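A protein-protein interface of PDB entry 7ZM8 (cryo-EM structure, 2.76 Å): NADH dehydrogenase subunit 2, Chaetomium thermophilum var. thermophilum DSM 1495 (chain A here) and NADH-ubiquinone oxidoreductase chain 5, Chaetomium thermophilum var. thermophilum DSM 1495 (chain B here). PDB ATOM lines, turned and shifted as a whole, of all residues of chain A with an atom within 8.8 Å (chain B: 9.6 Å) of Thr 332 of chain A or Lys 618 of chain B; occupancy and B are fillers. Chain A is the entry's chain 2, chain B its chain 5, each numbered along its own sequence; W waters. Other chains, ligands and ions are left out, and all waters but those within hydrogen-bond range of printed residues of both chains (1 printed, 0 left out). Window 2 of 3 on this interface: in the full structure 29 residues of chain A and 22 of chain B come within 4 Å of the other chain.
Thr 332 of chain A touches just these residues of chain B: Ser 617 and Lys 618.
Gly 330 of chain A touches none of the printed residues of chain B.
Printed residues of chain A within 4 Å of Ile 620 of chain B: Val 329 (3.6 Å).
Of the printed residues of chain B, Val 329 of chain A touches Ile 620.
Val 479 of chain A touches none of the printed residues of chain B.
The nearest residue of chain A that does not touch Lys 618 of chain B is Val 328 of chain A (6.3 Å).
Among the printed residues, pairs that only touch across the chains: Val 328 of chain A with Leu 616 of chain B (3.7 Å), Val 328 of chain A with Ser 617 of chain B (3.1 Å), Val 329 of chain A with Ile 620 of chain B (3.6 Å), Thr 332 of chain A with Lys 618 of chain B (3.9 Å), Gln 333 of chain A with Ser 621 of chain B (3.5 Å) and Arg 338 of chain A with Ser 624 of chain B (3.9 Å).
Water W1 lies within hydrogen-bond range of the side-chain hydroxyl (OH) of Tyr 342 of chain A (2.5 Å), the side-chain hydroxyl (OG) of Ser 621 of chain B (3.0 Å), the side-chain hydroxyl (OG) of Ser 624 of chain B (3.3 Å) and the guanidinium group (NH2) of Arg 338 of chain A (3.3 Å).
The side-chain hydroxyl (OG1) of Thr 332 of chain A lies close to the side-chain hydroxyl (OG) of Ser 617 of chain B.
O of Val 329 of chain A sits at hydrogen-bond distance from NE2 of Gln 333 of chain A.
The side-chain amide oxygen of Gln 333 of chain A is in hydrogen-bond range of the guanidinium group of Arg 338 of chain A (3.2 Å).
O of Leu 613 of chain B sits at hydrogen-bond distance from OG of Ser 617 of chain B.
O of Val 614 of chain B lies within hydrogen-bond range of OG of Ser 617 of chain B (3.2 Å).
The backbone carbonyl oxygen (O) of Ser 621 of chain B sits at hydrogen-bond distance from the side-chain hydroxyl (OG) of Ser 624 of chain B (2.8 Å).
Of the 20 printed residues of chain B, 6 touch a printed residue of chain A.
Printed residues of chain B that touch a printed residue of chain A: Leu 616, Ser 617, Lys 618, Ile 620, Ser 621 and Ser 624.
Hydrophobic or aromatic side chains of chain B that line the printed part of chain A: Leu 616 and Ile 620.
Of the 18 printed residues of chain A, 5 touch a printed residue of chain B.
Hydrophobic or aromatic side chains of chain A within 4 Å of the printed part of chain B: Val 328 and Val 329.
Among the printed residues, no Asp or Glu carboxylate lies within 4 Å of a Lys or Arg side-chain nitrogen of the other chain.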
ATOM      1  N   GLY A 326      25.510  -9.998  -3.196  1.00  0.00           N
ATOM      2  CA  GLY A 326      24.556  -9.143  -3.876  1.00  0.00           C
ATOM      3  C   GLY A 326      23.394  -9.901  -4.479  1.00  0.00           C
ATOM      4  O   GLY A 326      22.266  -9.403  -4.500  1.00  0.00           O
ATOM      5  N   THR A 327      23.641 -11.109  -4.968  1.00  0.00           N
ATOM      6  CA  THR A 327      22.586 -11.887  -5.597  1.00  0.00           C
ATOM      7  C   THR A 327      21.868 -12.814  -4.635  1.00  0.00           C
ATOM      8  O   THR A 327      20.675 -13.069  -4.819  1.00  0.00           O
ATOM      9  CB  THR A 327      23.146 -12.712  -6.758  1.00  0.00           C
ATOM     10  OG1 THR A 327      24.055 -13.697  -6.257  1.00  0.00           O
ATOM     11  CG2 THR A 327      23.860 -11.817  -7.749  1.00  0.00           C
ATOM     12  N   VAL A 328      22.549 -13.319  -3.610  1.00  0.00           N
ATOM     13  CA  VAL A 328      21.914 -14.293  -2.729  1.00  0.00           C
ATOM     14  C   VAL A 328      21.073 -13.599  -1.672  1.00  0.00           C
ATOM     15  O   VAL A 328      19.929 -13.987  -1.422  1.00  0.00           O
ATOM     16  CB  VAL A 328      22.969 -15.225  -2.107  1.00  0.00           C
ATOM     17  CG1 VAL A 328      22.431 -15.866  -0.847  1.00  0.00           C
ATOM     18  CG2 VAL A 328      23.350 -16.295  -3.100  1.00  0.00           C
ATOM     19  N   VAL A 329      21.612 -12.551  -1.047  1.00  0.00           N
ATOM     20  CA  VAL A 329      20.857 -11.851  -0.012  1.00  0.00           C
ATOM     21  C   VAL A 329      19.656 -11.127  -0.604  1.00  0.00           C
ATOM     22  O   VAL A 329      18.646 -10.926   0.081  1.00  0.00           O
ATOM     23  CB  VAL A 329      21.774 -10.889   0.763  1.00  0.00           C
ATOM     24  CG1 VAL A 329      21.036 -10.295   1.942  1.00  0.00           C
ATOM     25  CG2 VAL A 329      23.002 -11.624   1.237  1.00  0.00           C
ATOM     26  N   GLY A 330      19.725 -10.739  -1.874  1.00  0.00           N
ATOM     27  CA  GLY A 330      18.627 -10.021  -2.492  1.00  0.00           C
ATOM     28  C   GLY A 330      17.369 -10.835  -2.700  1.00  0.00           C
ATOM     29  O   GLY A 330      16.323 -10.251  -2.996  1.00  0.00           O
ATOM     30  N   LEU A 331      17.439 -12.156  -2.540  1.00  0.00           N
ATOM     31  CA  LEU A 331      16.304 -13.010  -2.870  1.00  0.00           C
ATOM     32  C   LEU A 331      15.105 -12.739  -1.973  1.00  0.00           C
ATOM     33  O   LEU A 331      13.960 -12.761  -2.436  1.00  0.00           O
ATOM     34  CB  LEU A 331      16.717 -14.474  -2.778  1.00  0.00           C
ATOM     35  CG  LEU A 331      17.663 -14.936  -3.877  1.00  0.00           C
ATOM     36  CD1 LEU A 331      18.000 -16.397  -3.706  1.00  0.00           C
ATOM     37  CD2 LEU A 331      17.027 -14.685  -5.219  1.00  0.00           C
ATOM     38  N   THR A 332      15.339 -12.491  -0.687  1.00  0.00           N
ATOM     39  CA  THR A 332      14.263 -12.355   0.286  1.00  0.00           C
ATOM     40  C   THR A 332      13.991 -10.904   0.665  1.00  0.00           C
ATOM     41  O   THR A 332      13.423 -10.637   1.726  1.00  0.00           O
ATOM     42  CB  THR A 332      14.569 -13.173   1.539  1.00  0.00           C
ATOM     43  OG1 THR A 332      15.931 -12.961   1.923  1.00  0.00           O
ATOM     44  CG2 THR A 332      14.325 -14.649   1.290  1.00  0.00           C
ATOM     45  N   GLN A 333      14.377  -9.958  -0.171  1.00  0.00           N
ATOM     46  CA  GLN A 333      14.086  -8.563   0.097  1.00  0.00           C
ATOM     47  C   GLN A 333      12.684  -8.241  -0.396  1.00  0.00           C
ATOM     48  O   GLN A 333      12.296  -8.651  -1.492  1.00  0.00           O
ATOM     49  CB  GLN A 333      15.119  -7.652  -0.570  1.00  0.00           C
ATOM     50  CG  GLN A 333      16.547  -7.939  -0.148  1.00  0.00           C
ATOM     51  CD  GLN A 333      16.767  -7.740   1.337  1.00  0.00           C
ATOM     52  OE1 GLN A 333      16.792  -6.614   1.822  1.00  0.00           O
ATOM     53  NE2 GLN A 333      16.925  -8.835   2.067  1.00  0.00           N
ATOM     54  N   PHE A 334      11.917  -7.539   0.432  1.00  0.00           N
ATOM     55  CA  PHE A 334      10.594  -7.080   0.051  1.00  0.00           C
ATOM     56  C   PHE A 334      10.502  -5.567  -0.050  1.00  0.00           C
ATOM     57  O   PHE A 334       9.472  -5.055  -0.496  1.00  0.00           O
ATOM     58  CB  PHE A 334       9.542  -7.595   1.043  1.00  0.00           C
ATOM     59  CG  PHE A 334       9.665  -7.003   2.405  1.00  0.00           C
ATOM     60  CD1 PHE A 334      10.545  -7.536   3.320  1.00  0.00           C
ATOM     61  CD2 PHE A 334       8.911  -5.907   2.769  1.00  0.00           C
ATOM     62  CE1 PHE A 334      10.672  -6.993   4.554  1.00  0.00           C
ATOM     63  CE2 PHE A 334       9.040  -5.361   4.009  1.00  0.00           C
ATOM     64  CZ  PHE A 334       9.924  -5.906   4.901  1.00  0.00           C
ATOM     65  N   ARG A 335      11.539  -4.845   0.346  1.00  0.00           N
ATOM     66  CA  ARG A 335      11.586  -3.398   0.224  1.00  0.00           C
ATOM     67  C   ARG A 335      12.416  -3.030  -1.000  1.00  0.00           C
ATOM     68  O   ARG A 335      13.524  -3.538  -1.178  1.00  0.00           O
ATOM     69  CB  ARG A 335      12.157  -2.771   1.496  1.00  0.00           C
ATOM     70  CG  ARG A 335      11.226  -2.914   2.684  1.00  0.00           C
ATOM     71  CD  ARG A 335      11.687  -2.141   3.892  1.00  0.00           C
ATOM     72  NE  ARG A 335      11.688  -0.706   3.660  1.00  0.00           N
ATOM     73  CZ  ARG A 335      10.671   0.100   3.925  1.00  0.00           C
ATOM     74  NH1 ARG A 335      10.779   1.391   3.674  1.00  0.00           N
ATOM     75  NH2 ARG A 335       9.555  -0.380   4.443  1.00  0.00           N
ATOM     76  N   ARG A 338      15.965  -1.448  -0.545  1.00  0.00           N
ATOM     77  CA  ARG A 338      16.912  -2.463  -0.096  1.00  0.00           C
ATOM     78  C   ARG A 338      17.294  -3.394  -1.236  1.00  0.00           C
ATOM     79  O   ARG A 338      18.444  -3.831  -1.332  1.00  0.00           O
ATOM     80  CB  ARG A 338      16.327  -3.263   1.065  1.00  0.00           C
ATOM     81  CG  ARG A 338      15.969  -2.433   2.265  1.00  0.00           C
ATOM     82  CD  ARG A 338      15.745  -3.294   3.482  1.00  0.00           C
ATOM     83  NE  ARG A 338      16.902  -4.123   3.788  1.00  0.00           N
ATOM     84  CZ  ARG A 338      17.893  -3.754   4.589  1.00  0.00           C
ATOM     85  NH1 ARG A 338      17.874  -2.560   5.165  1.00  0.00           N
ATOM     86  NH2 ARG A 338      18.908  -4.575   4.807  1.00  0.00           N
ATOM     87  N   LEU A 339      16.335  -3.717  -2.105  1.00  0.00           N
ATOM     88  CA  LEU A 339      16.625  -4.565  -3.251  1.00  0.00           C
ATOM     89  C   LEU A 339      17.577  -3.887  -4.222  1.00  0.00           C
ATOM     90  O   LEU A 339      18.512  -4.518  -4.725  1.00  0.00           O
ATOM     91  CB  LEU A 339      15.332  -4.941  -3.964  1.00  0.00           C
ATOM     92  CG  LEU A 339      15.529  -5.978  -5.064  1.00  0.00           C
ATOM     93  CD1 LEU A 339      15.726  -7.329  -4.438  1.00  0.00           C
ATOM     94  CD2 LEU A 339      14.367  -5.998  -6.009  1.00  0.00           C
ATOM     95  N   TYR A 342      21.144  -3.920  -2.907  1.00  0.00           N
ATOM     96  CA  TYR A 342      21.840  -5.186  -3.100  1.00  0.00           C
ATOM     97  C   TYR A 342      22.145  -5.438  -4.567  1.00  0.00           C
ATOM     98  O   TYR A 342      23.154  -6.071  -4.890  1.00  0.00           O
ATOM     99  CB  TYR A 342      21.019  -6.336  -2.521  1.00  0.00           C
ATOM    100  CG  TYR A 342      21.161  -6.484  -1.029  1.00  0.00           C
ATOM    101  CD1 TYR A 342      22.344  -6.934  -0.468  1.00  0.00           C
ATOM    102  CD2 TYR A 342      20.114  -6.163  -0.177  1.00  0.00           C
ATOM    103  CE1 TYR A 342      22.478  -7.060   0.893  1.00  0.00           C
ATOM    104  CE2 TYR A 342      20.240  -6.289   1.183  1.00  0.00           C
ATOM    105  CZ  TYR A 342      21.424  -6.737   1.711  1.00  0.00           C
ATOM    106  OH  TYR A 342      21.554  -6.863   3.070  1.00  0.00           O
ATOM    107  N   ILE A 415       7.788  -3.468  -2.805  1.00  0.00           N
ATOM    108  CA  ILE A 415       7.535  -4.034  -4.120  1.00  0.00           C
ATOM    109  C   ILE A 415       6.063  -4.396  -4.278  1.00  0.00           C
ATOM    110  O   ILE A 415       5.552  -4.440  -5.400  1.00  0.00           O
ATOM    111  CB  ILE A 415       8.476  -5.232  -4.327  1.00  0.00           C
ATOM    112  CG1 ILE A 415       9.922  -4.774  -4.131  1.00  0.00           C
ATOM    113  CG2 ILE A 415       8.288  -5.858  -5.701  1.00  0.00           C
ATOM    114  CD1 ILE A 415      10.879  -5.861  -3.747  1.00  0.00           C
ATOM    115  N   ILE A 476      21.092 -16.357 -10.182  1.00  0.00           N
ATOM    116  CA  ILE A 476      20.509 -16.152  -8.858  1.00  0.00           C
ATOM    117  C   ILE A 476      19.988 -14.731  -8.719  1.00  0.00           C
ATOM    118  O   ILE A 476      18.889 -14.507  -8.204  1.00  0.00           O
ATOM    119  CB  ILE A 476      21.532 -16.487  -7.757  1.00  0.00           C
ATOM    120  CG1 ILE A 476      22.001 -17.936  -7.881  1.00  0.00           C
ATOM    121  CG2 ILE A 476      20.935 -16.245  -6.378  1.00  0.00           C
ATOM    122  CD1 ILE A 476      23.188 -18.258  -7.014  1.00  0.00           C
ATOM    123  N   VAL A 479      16.652 -13.837 -10.264  1.00  0.00           N
ATOM    124  CA  VAL A 479      15.430 -14.281  -9.606  1.00  0.00           C
ATOM    125  C   VAL A 479      14.707 -13.101  -8.972  1.00  0.00           C
ATOM    126  O   VAL A 479      13.499 -12.927  -9.153  1.00  0.00           O
ATOM    127  CB  VAL A 479      15.744 -15.369  -8.568  1.00  0.00           C
ATOM    128  CG1 VAL A 479      14.501 -15.715  -7.773  1.00  0.00           C
ATOM    129  CG2 VAL A 479      16.321 -16.597  -9.237  1.00  0.00           C
ATOM    130  N   TYR A 480      15.430 -12.266  -8.224  1.00  0.00           N
ATOM    131  CA  TYR A 480      14.762 -11.153  -7.566  1.00  0.00           C
ATOM    132  C   TYR A 480      14.458 -10.012  -8.525  1.00  0.00           C
ATOM    133  O   TYR A 480      13.580  -9.198  -8.233  1.00  0.00           O
ATOM    134  CB  TYR A 480      15.571 -10.661  -6.353  1.00  0.00           C
ATOM    135  CG  TYR A 480      16.950 -10.081  -6.599  1.00  0.00           C
ATOM    136  CD1 TYR A 480      17.119  -8.857  -7.237  1.00  0.00           C
ATOM    137  CD2 TYR A 480      18.083 -10.739  -6.149  1.00  0.00           C
ATOM    138  CE1 TYR A 480      18.372  -8.326  -7.439  1.00  0.00           C
ATOM    139  CE2 TYR A 480      19.338 -10.215  -6.349  1.00  0.00           C
ATOM    140  CZ  TYR A 480      19.478  -9.009  -6.992  1.00  0.00           C
ATOM    141  OH  TYR A 480      20.734  -8.492  -7.189  1.00  0.00           O
ATOM    142  N   ASN A 483      11.057 -11.145  -9.901  1.00  0.00           N
ATOM    143  CA  ASN A 483       9.982 -11.023  -8.888  1.00  0.00           C
ATOM    144  C   ASN A 483       9.372  -9.615  -8.960  1.00  0.00           C
ATOM    145  O   ASN A 483       8.161  -9.485  -8.784  1.00  0.00           O
ATOM    146  CB  ASN A 483      10.515 -11.465  -7.521  1.00  0.00           C
ATOM    147  CG  ASN A 483      10.419 -12.957  -7.303  1.00  0.00           C
ATOM    148  OD1 ASN A 483       9.358 -13.550  -7.477  1.00  0.00           O
ATOM    149  ND2 ASN A 483      11.517 -13.575  -6.909  1.00  0.00           N
ATOM    150  N   GLU B 610      15.763 -23.690  -4.696  1.00  0.00           N
ATOM    151  CA  GLU B 610      14.866 -22.653  -4.200  1.00  0.00           C
ATOM    152  C   GLU B 610      14.784 -22.663  -2.681  1.00  0.00           C
ATOM    153  O   GLU B 610      15.018 -21.641  -2.027  1.00  0.00           O
ATOM    154  CB  GLU B 610      13.470 -22.845  -4.787  1.00  0.00           C
ATOM    155  CG  GLU B 610      12.489 -21.766  -4.379  1.00  0.00           C
ATOM    156  CD  GLU B 610      11.126 -21.947  -5.004  1.00  0.00           C
ATOM    157  OE1 GLU B 610      10.945 -22.932  -5.743  1.00  0.00           O
ATOM    158  OE2 GLU B 610      10.234 -21.111  -4.752  1.00  0.00           O
ATOM    159  N   ARG B 611      14.442 -23.826  -2.124  1.00  0.00           N
ATOM    160  CA  ARG B 611      14.210 -23.921  -0.666  1.00  0.00           C
ATOM    161  C   ARG B 611      15.535 -23.844   0.083  1.00  0.00           C
ATOM    162  O   ARG B 611      15.536 -23.386   1.229  1.00  0.00           O
ATOM    163  CB  ARG B 611      13.433 -25.215  -0.381  1.00  0.00           C
ATOM    164  CG  ARG B 611      14.246 -26.488  -0.534  1.00  0.00           C
ATOM    165  CD  ARG B 611      13.388 -27.728  -0.448  1.00  0.00           C
ATOM    166  NE  ARG B 611      12.609 -27.733   0.775  1.00  0.00           N
ATOM    167  CZ  ARG B 611      12.014 -28.806   1.274  1.00  0.00           C
ATOM    168  NH1 ARG B 611      11.317 -28.716   2.393  1.00  0.00           N
ATOM    169  NH2 ARG B 611      12.131 -29.969   0.660  1.00  0.00           N
ATOM    170  N   GLY B 612      16.624 -24.249  -0.552  1.00  0.00           N
ATOM    171  CA  GLY B 612      17.945 -24.118   0.089  1.00  0.00           C
ATOM    172  C   GLY B 612      18.411 -22.682   0.129  1.00  0.00           C
ATOM    173  O   GLY B 612      18.859 -22.244   1.192  1.00  0.00           O
ATOM    174  N   LEU B 613      18.284 -21.963  -0.982  1.00  0.00           N
ATOM    175  CA  LEU B 613      18.807 -20.603  -1.058  1.00  0.00           C
ATOM    176  C   LEU B 613      17.956 -19.628  -0.258  1.00  0.00           C
ATOM    177  O   LEU B 613      18.486 -18.693   0.351  1.00  0.00           O
ATOM    178  CB  LEU B 613      18.900 -20.155  -2.514  1.00  0.00           C
ATOM    179  CG  LEU B 613      20.168 -20.541  -3.271  1.00  0.00           C
ATOM    180  CD1 LEU B 613      20.196 -19.874  -4.619  1.00  0.00           C
ATOM    181  CD2 LEU B 613      21.400 -20.181  -2.472  1.00  0.00           C
ATOM    182  N   VAL B 614      16.637 -19.814  -0.261  1.00  0.00           N
ATOM    183  CA  VAL B 614      15.761 -18.931   0.503  1.00  0.00           C
ATOM    184  C   VAL B 614      16.060 -19.049   1.989  1.00  0.00           C
ATOM    185  O   VAL B 614      16.010 -18.062   2.732  1.00  0.00           O
ATOM    186  CB  VAL B 614      14.286 -19.243   0.188  1.00  0.00           C
ATOM    187  CG1 VAL B 614      13.381 -18.717   1.279  1.00  0.00           C
ATOM    188  CG2 VAL B 614      13.902 -18.650  -1.144  1.00  0.00           C
ATOM    189  N   LYS B 615      16.368 -20.260   2.450  1.00  0.00           N
ATOM    190  CA  LYS B 615      16.780 -20.439   3.834  1.00  0.00           C
ATOM    191  C   LYS B 615      18.106 -19.740   4.104  1.00  0.00           C
ATOM    192  O   LYS B 615      18.271 -19.075   5.131  1.00  0.00           O
ATOM    193  CB  LYS B 615      16.879 -21.926   4.151  1.00  0.00           C
ATOM    194  CG  LYS B 615      17.061 -22.243   5.611  1.00  0.00           C
ATOM    195  CD  LYS B 615      17.401 -23.708   5.801  1.00  0.00           C
ATOM    196  CE  LYS B 615      16.169 -24.519   6.166  1.00  0.00           C
ATOM    197  NZ  LYS B 615      15.647 -24.155   7.511  1.00  0.00           N
ATOM    198  N   LEU B 616      19.061 -19.878   3.185  1.00  0.00           N
ATOM    199  CA  LEU B 616      20.360 -19.242   3.353  1.00  0.00           C
ATOM    200  C   LEU B 616      20.236 -17.727   3.370  1.00  0.00           C
ATOM    201  O   LEU B 616      20.850 -17.056   4.205  1.00  0.00           O
ATOM    202  CB  LEU B 616      21.295 -19.696   2.233  1.00  0.00           C
ATOM    203  CG  LEU B 616      22.548 -18.879   1.935  1.00  0.00           C
ATOM    204  CD1 LEU B 616      23.608 -19.172   2.948  1.00  0.00           C
ATOM    205  CD2 LEU B 616      23.060 -19.183   0.555  1.00  0.00           C
ATOM    206  N   SER B 617      19.434 -17.170   2.460  1.00  0.00           N
ATOM    207  CA  SER B 617      19.360 -15.721   2.317  1.00  0.00           C
ATOM    208  C   SER B 617      18.663 -15.066   3.496  1.00  0.00           C
ATOM    209  O   SER B 617      18.918 -13.893   3.783  1.00  0.00           O
ATOM    210  CB  SER B 617      18.651 -15.358   1.017  1.00  0.00           C
ATOM    211  OG  SER B 617      17.291 -15.728   1.046  1.00  0.00           O
ATOM    212  N   LYS B 618      17.775 -15.790   4.175  1.00  0.00           N
ATOM    213  CA  LYS B 618      17.141 -15.245   5.368  1.00  0.00           C
ATOM    214  C   LYS B 618      18.129 -15.156   6.523  1.00  0.00           C
ATOM    215  O   LYS B 618      18.038 -14.251   7.357  1.00  0.00           O
ATOM    216  CB  LYS B 618      15.939 -16.098   5.758  1.00  0.00           C
ATOM    217  CG  LYS B 618      14.675 -15.751   5.026  1.00  0.00           C
ATOM    218  CD  LYS B 618      13.490 -16.430   5.661  1.00  0.00           C
ATOM    219  CE  LYS B 618      13.627 -17.938   5.580  1.00  0.00           C
ATOM    220  NZ  LYS B 618      12.359 -18.629   5.912  1.00  0.00           N
ATOM    221  N   ASN B 619      19.067 -16.097   6.596  1.00  0.00           N
ATOM    222  CA  ASN B 619      20.046 -16.101   7.672  1.00  0.00           C
ATOM    223  C   ASN B 619      21.055 -14.972   7.506  1.00  0.00           C
ATOM    224  O   ASN B 619      21.360 -14.256   8.466  1.00  0.00           O
ATOM    225  CB  ASN B 619      20.748 -17.454   7.721  1.00  0.00           C
ATOM    226  CG  ASN B 619      19.811 -18.579   8.107  1.00  0.00           C
ATOM    227  OD1 ASN B 619      19.029 -18.454   9.044  1.00  0.00           O
ATOM    228  ND2 ASN B 619      19.878 -19.682   7.378  1.00  0.00           N
ATOM    229  N   ILE B 620      21.594 -14.802   6.298  1.00  0.00           N
ATOM    230  CA  ILE B 620      22.519 -13.701   6.054  1.00  0.00           C
ATOM    231  C   ILE B 620      21.810 -12.369   6.237  1.00  0.00           C
ATOM    232  O   ILE B 620      22.375 -11.415   6.778  1.00  0.00           O
ATOM    233  CB  ILE B 620      23.144 -13.816   4.652  1.00  0.00           C
ATOM    234  CG1 ILE B 620      23.750 -15.198   4.435  1.00  0.00           C
ATOM    235  CG2 ILE B 620      24.201 -12.753   4.451  1.00  0.00           C
ATOM    236  CD1 ILE B 620      24.159 -15.454   3.010  1.00  0.00           C
ATOM    237  N   SER B 621      20.560 -12.281   5.780  1.00  0.00           N
ATOM    238  CA  SER B 621      19.794 -11.056   5.940  1.00  0.00           C
ATOM    239  C   SER B 621      19.485 -10.757   7.398  1.00  0.00           C
ATOM    240  O   SER B 621      19.159  -9.614   7.727  1.00  0.00           O
ATOM    241  CB  SER B 621      18.499 -11.143   5.139  1.00  0.00           C
ATOM    242  OG  SER B 621      17.722  -9.976   5.303  1.00  0.00           O
ATOM    243  N   SER B 622      19.583 -11.751   8.274  1.00  0.00           N
ATOM    244  CA  SER B 622      19.392 -11.540   9.700  1.00  0.00           C
ATOM    245  C   SER B 622      20.658 -11.078  10.404  1.00  0.00           C
ATOM    246  O   SER B 622      20.620 -10.833  11.613  1.00  0.00           O
ATOM    247  CB  SER B 622      18.878 -12.822  10.354  1.00  0.00           C
ATOM    248  OG  SER B 622      19.923 -13.760  10.526  1.00  0.00           O
ATOM    249  N   LEU B 623      21.776 -10.967   9.685  1.00  0.00           N
ATOM    250  CA  LEU B 623      22.970 -10.358  10.257  1.00  0.00           C
ATOM    251  C   LEU B 623      22.874  -8.840  10.269  1.00  0.00           C
ATOM    252  O   LEU B 623      23.665  -8.178  10.947  1.00  0.00           O
ATOM    253  CB  LEU B 623      24.209 -10.795   9.480  1.00  0.00           C
ATOM    254  CG  LEU B 623      24.633 -12.256   9.591  1.00  0.00           C
ATOM    255  CD1 LEU B 623      25.565 -12.623   8.452  1.00  0.00           C
ATOM    256  CD2 LEU B 623      25.294 -12.512  10.926  1.00  0.00           C
ATOM    257  N   SER B 624      21.925  -8.274   9.530  1.00  0.00           N
ATOM    258  CA  SER B 624      21.836  -6.829   9.333  1.00  0.00           C
ATOM    259  C   SER B 624      20.803  -6.257  10.290  1.00  0.00           C
ATOM    260  O   SER B 624      19.615  -6.192   9.970  1.00  0.00           O
ATOM    261  CB  SER B 624      21.480  -6.513   7.887  1.00  0.00           C
ATOM    262  OG  SER B 624      20.175  -6.973   7.587  1.00  0.00           O
ATOM    263  N   MET B 666      25.379 -20.615   7.301  1.00  0.00           N
ATOM    264  CA  MET B 666      24.123 -19.898   7.138  1.00  0.00           C
ATOM    265  C   MET B 666      23.043 -20.758   6.498  1.00  0.00           C
ATOM    266  O   MET B 666      21.874 -20.362   6.497  1.00  0.00           O
ATOM    267  CB  MET B 666      24.341 -18.641   6.294  1.00  0.00           C
ATOM    268  CG  MET B 666      25.231 -17.572   6.919  1.00  0.00           C
ATOM    269  SD  MET B 666      24.588 -16.898   8.462  1.00  0.00           S
ATOM    270  CE  MET B 666      25.601 -17.759   9.664  1.00  0.00           C
ATOM    271  N   MET B 667      23.397 -21.936   5.982  1.00  0.00           N
ATOM    272  CA  MET B 667      22.409 -22.885   5.402  1.00  0.00           C
ATOM    273  C   MET B 667      21.694 -23.610   6.548  1.00  0.00           C
ATOM    274  O   MET B 667      20.572 -24.092   6.329  1.00  0.00           O
ATOM    275  CB  MET B 667      23.126 -23.918   4.530  1.00  0.00           C
ATOM    276  CG  MET B 667      22.203 -24.734   3.652  1.00  0.00           C
ATOM    277  SD  MET B 667      21.420 -23.706   2.393  1.00  0.00           S
ATOM    278  CE  MET B 667      22.815 -23.372   1.319  1.00  0.00           C
ATOM    279  N   ILE B 668      22.322 -23.693   7.724  1.00  0.00           N
ATOM    280  CA  ILE B 668      21.729 -24.363   8.873  1.00  0.00           C
ATOM    281  C   ILE B 668      21.053 -23.316   9.745  1.00  0.00           C
ATOM    282  O   ILE B 668      21.651 -22.280  10.062  1.00  0.00           O
ATOM    283  CB  ILE B 668      22.786 -25.145   9.670  1.00  0.00           C
ATOM    284  CG1 ILE B 668      23.449 -26.197   8.780  1.00  0.00           C
ATOM    285  CG2 ILE B 668      22.159 -25.796  10.892  1.00  0.00           C
ATOM    286  CD1 ILE B 668      24.676 -26.826   9.397  1.00  0.00           C
ATOM    287  N   GLY B 669      19.803 -23.579  10.125  1.00  0.00           N
ATOM    288  CA  GLY B 669      19.052 -22.660  10.952  1.00  0.00           C
ATOM    289  C   GLY B 669      19.403 -22.774  12.422  1.00  0.00           C
ATOM    290  O   GLY B 669      20.184 -23.625  12.850  1.00  0.00           O
ATOM    291  N   GLU B 670      18.801 -21.881  13.206  1.00  0.00           N
ATOM    292  CA  GLU B 670      18.999 -21.826  14.653  1.00  0.00           C
ATOM    293  C   GLU B 670      20.474 -21.679  15.021  1.00  0.00           C
ATOM    294  O   GLU B 670      20.809 -21.160  16.085  1.00  0.00           O
ATOM    295  CB  GLU B 670      18.412 -23.071  15.324  1.00  0.00           C
HETATM  296  O   HOH W   1      19.647  -7.795   4.478  1.00  0.00           O
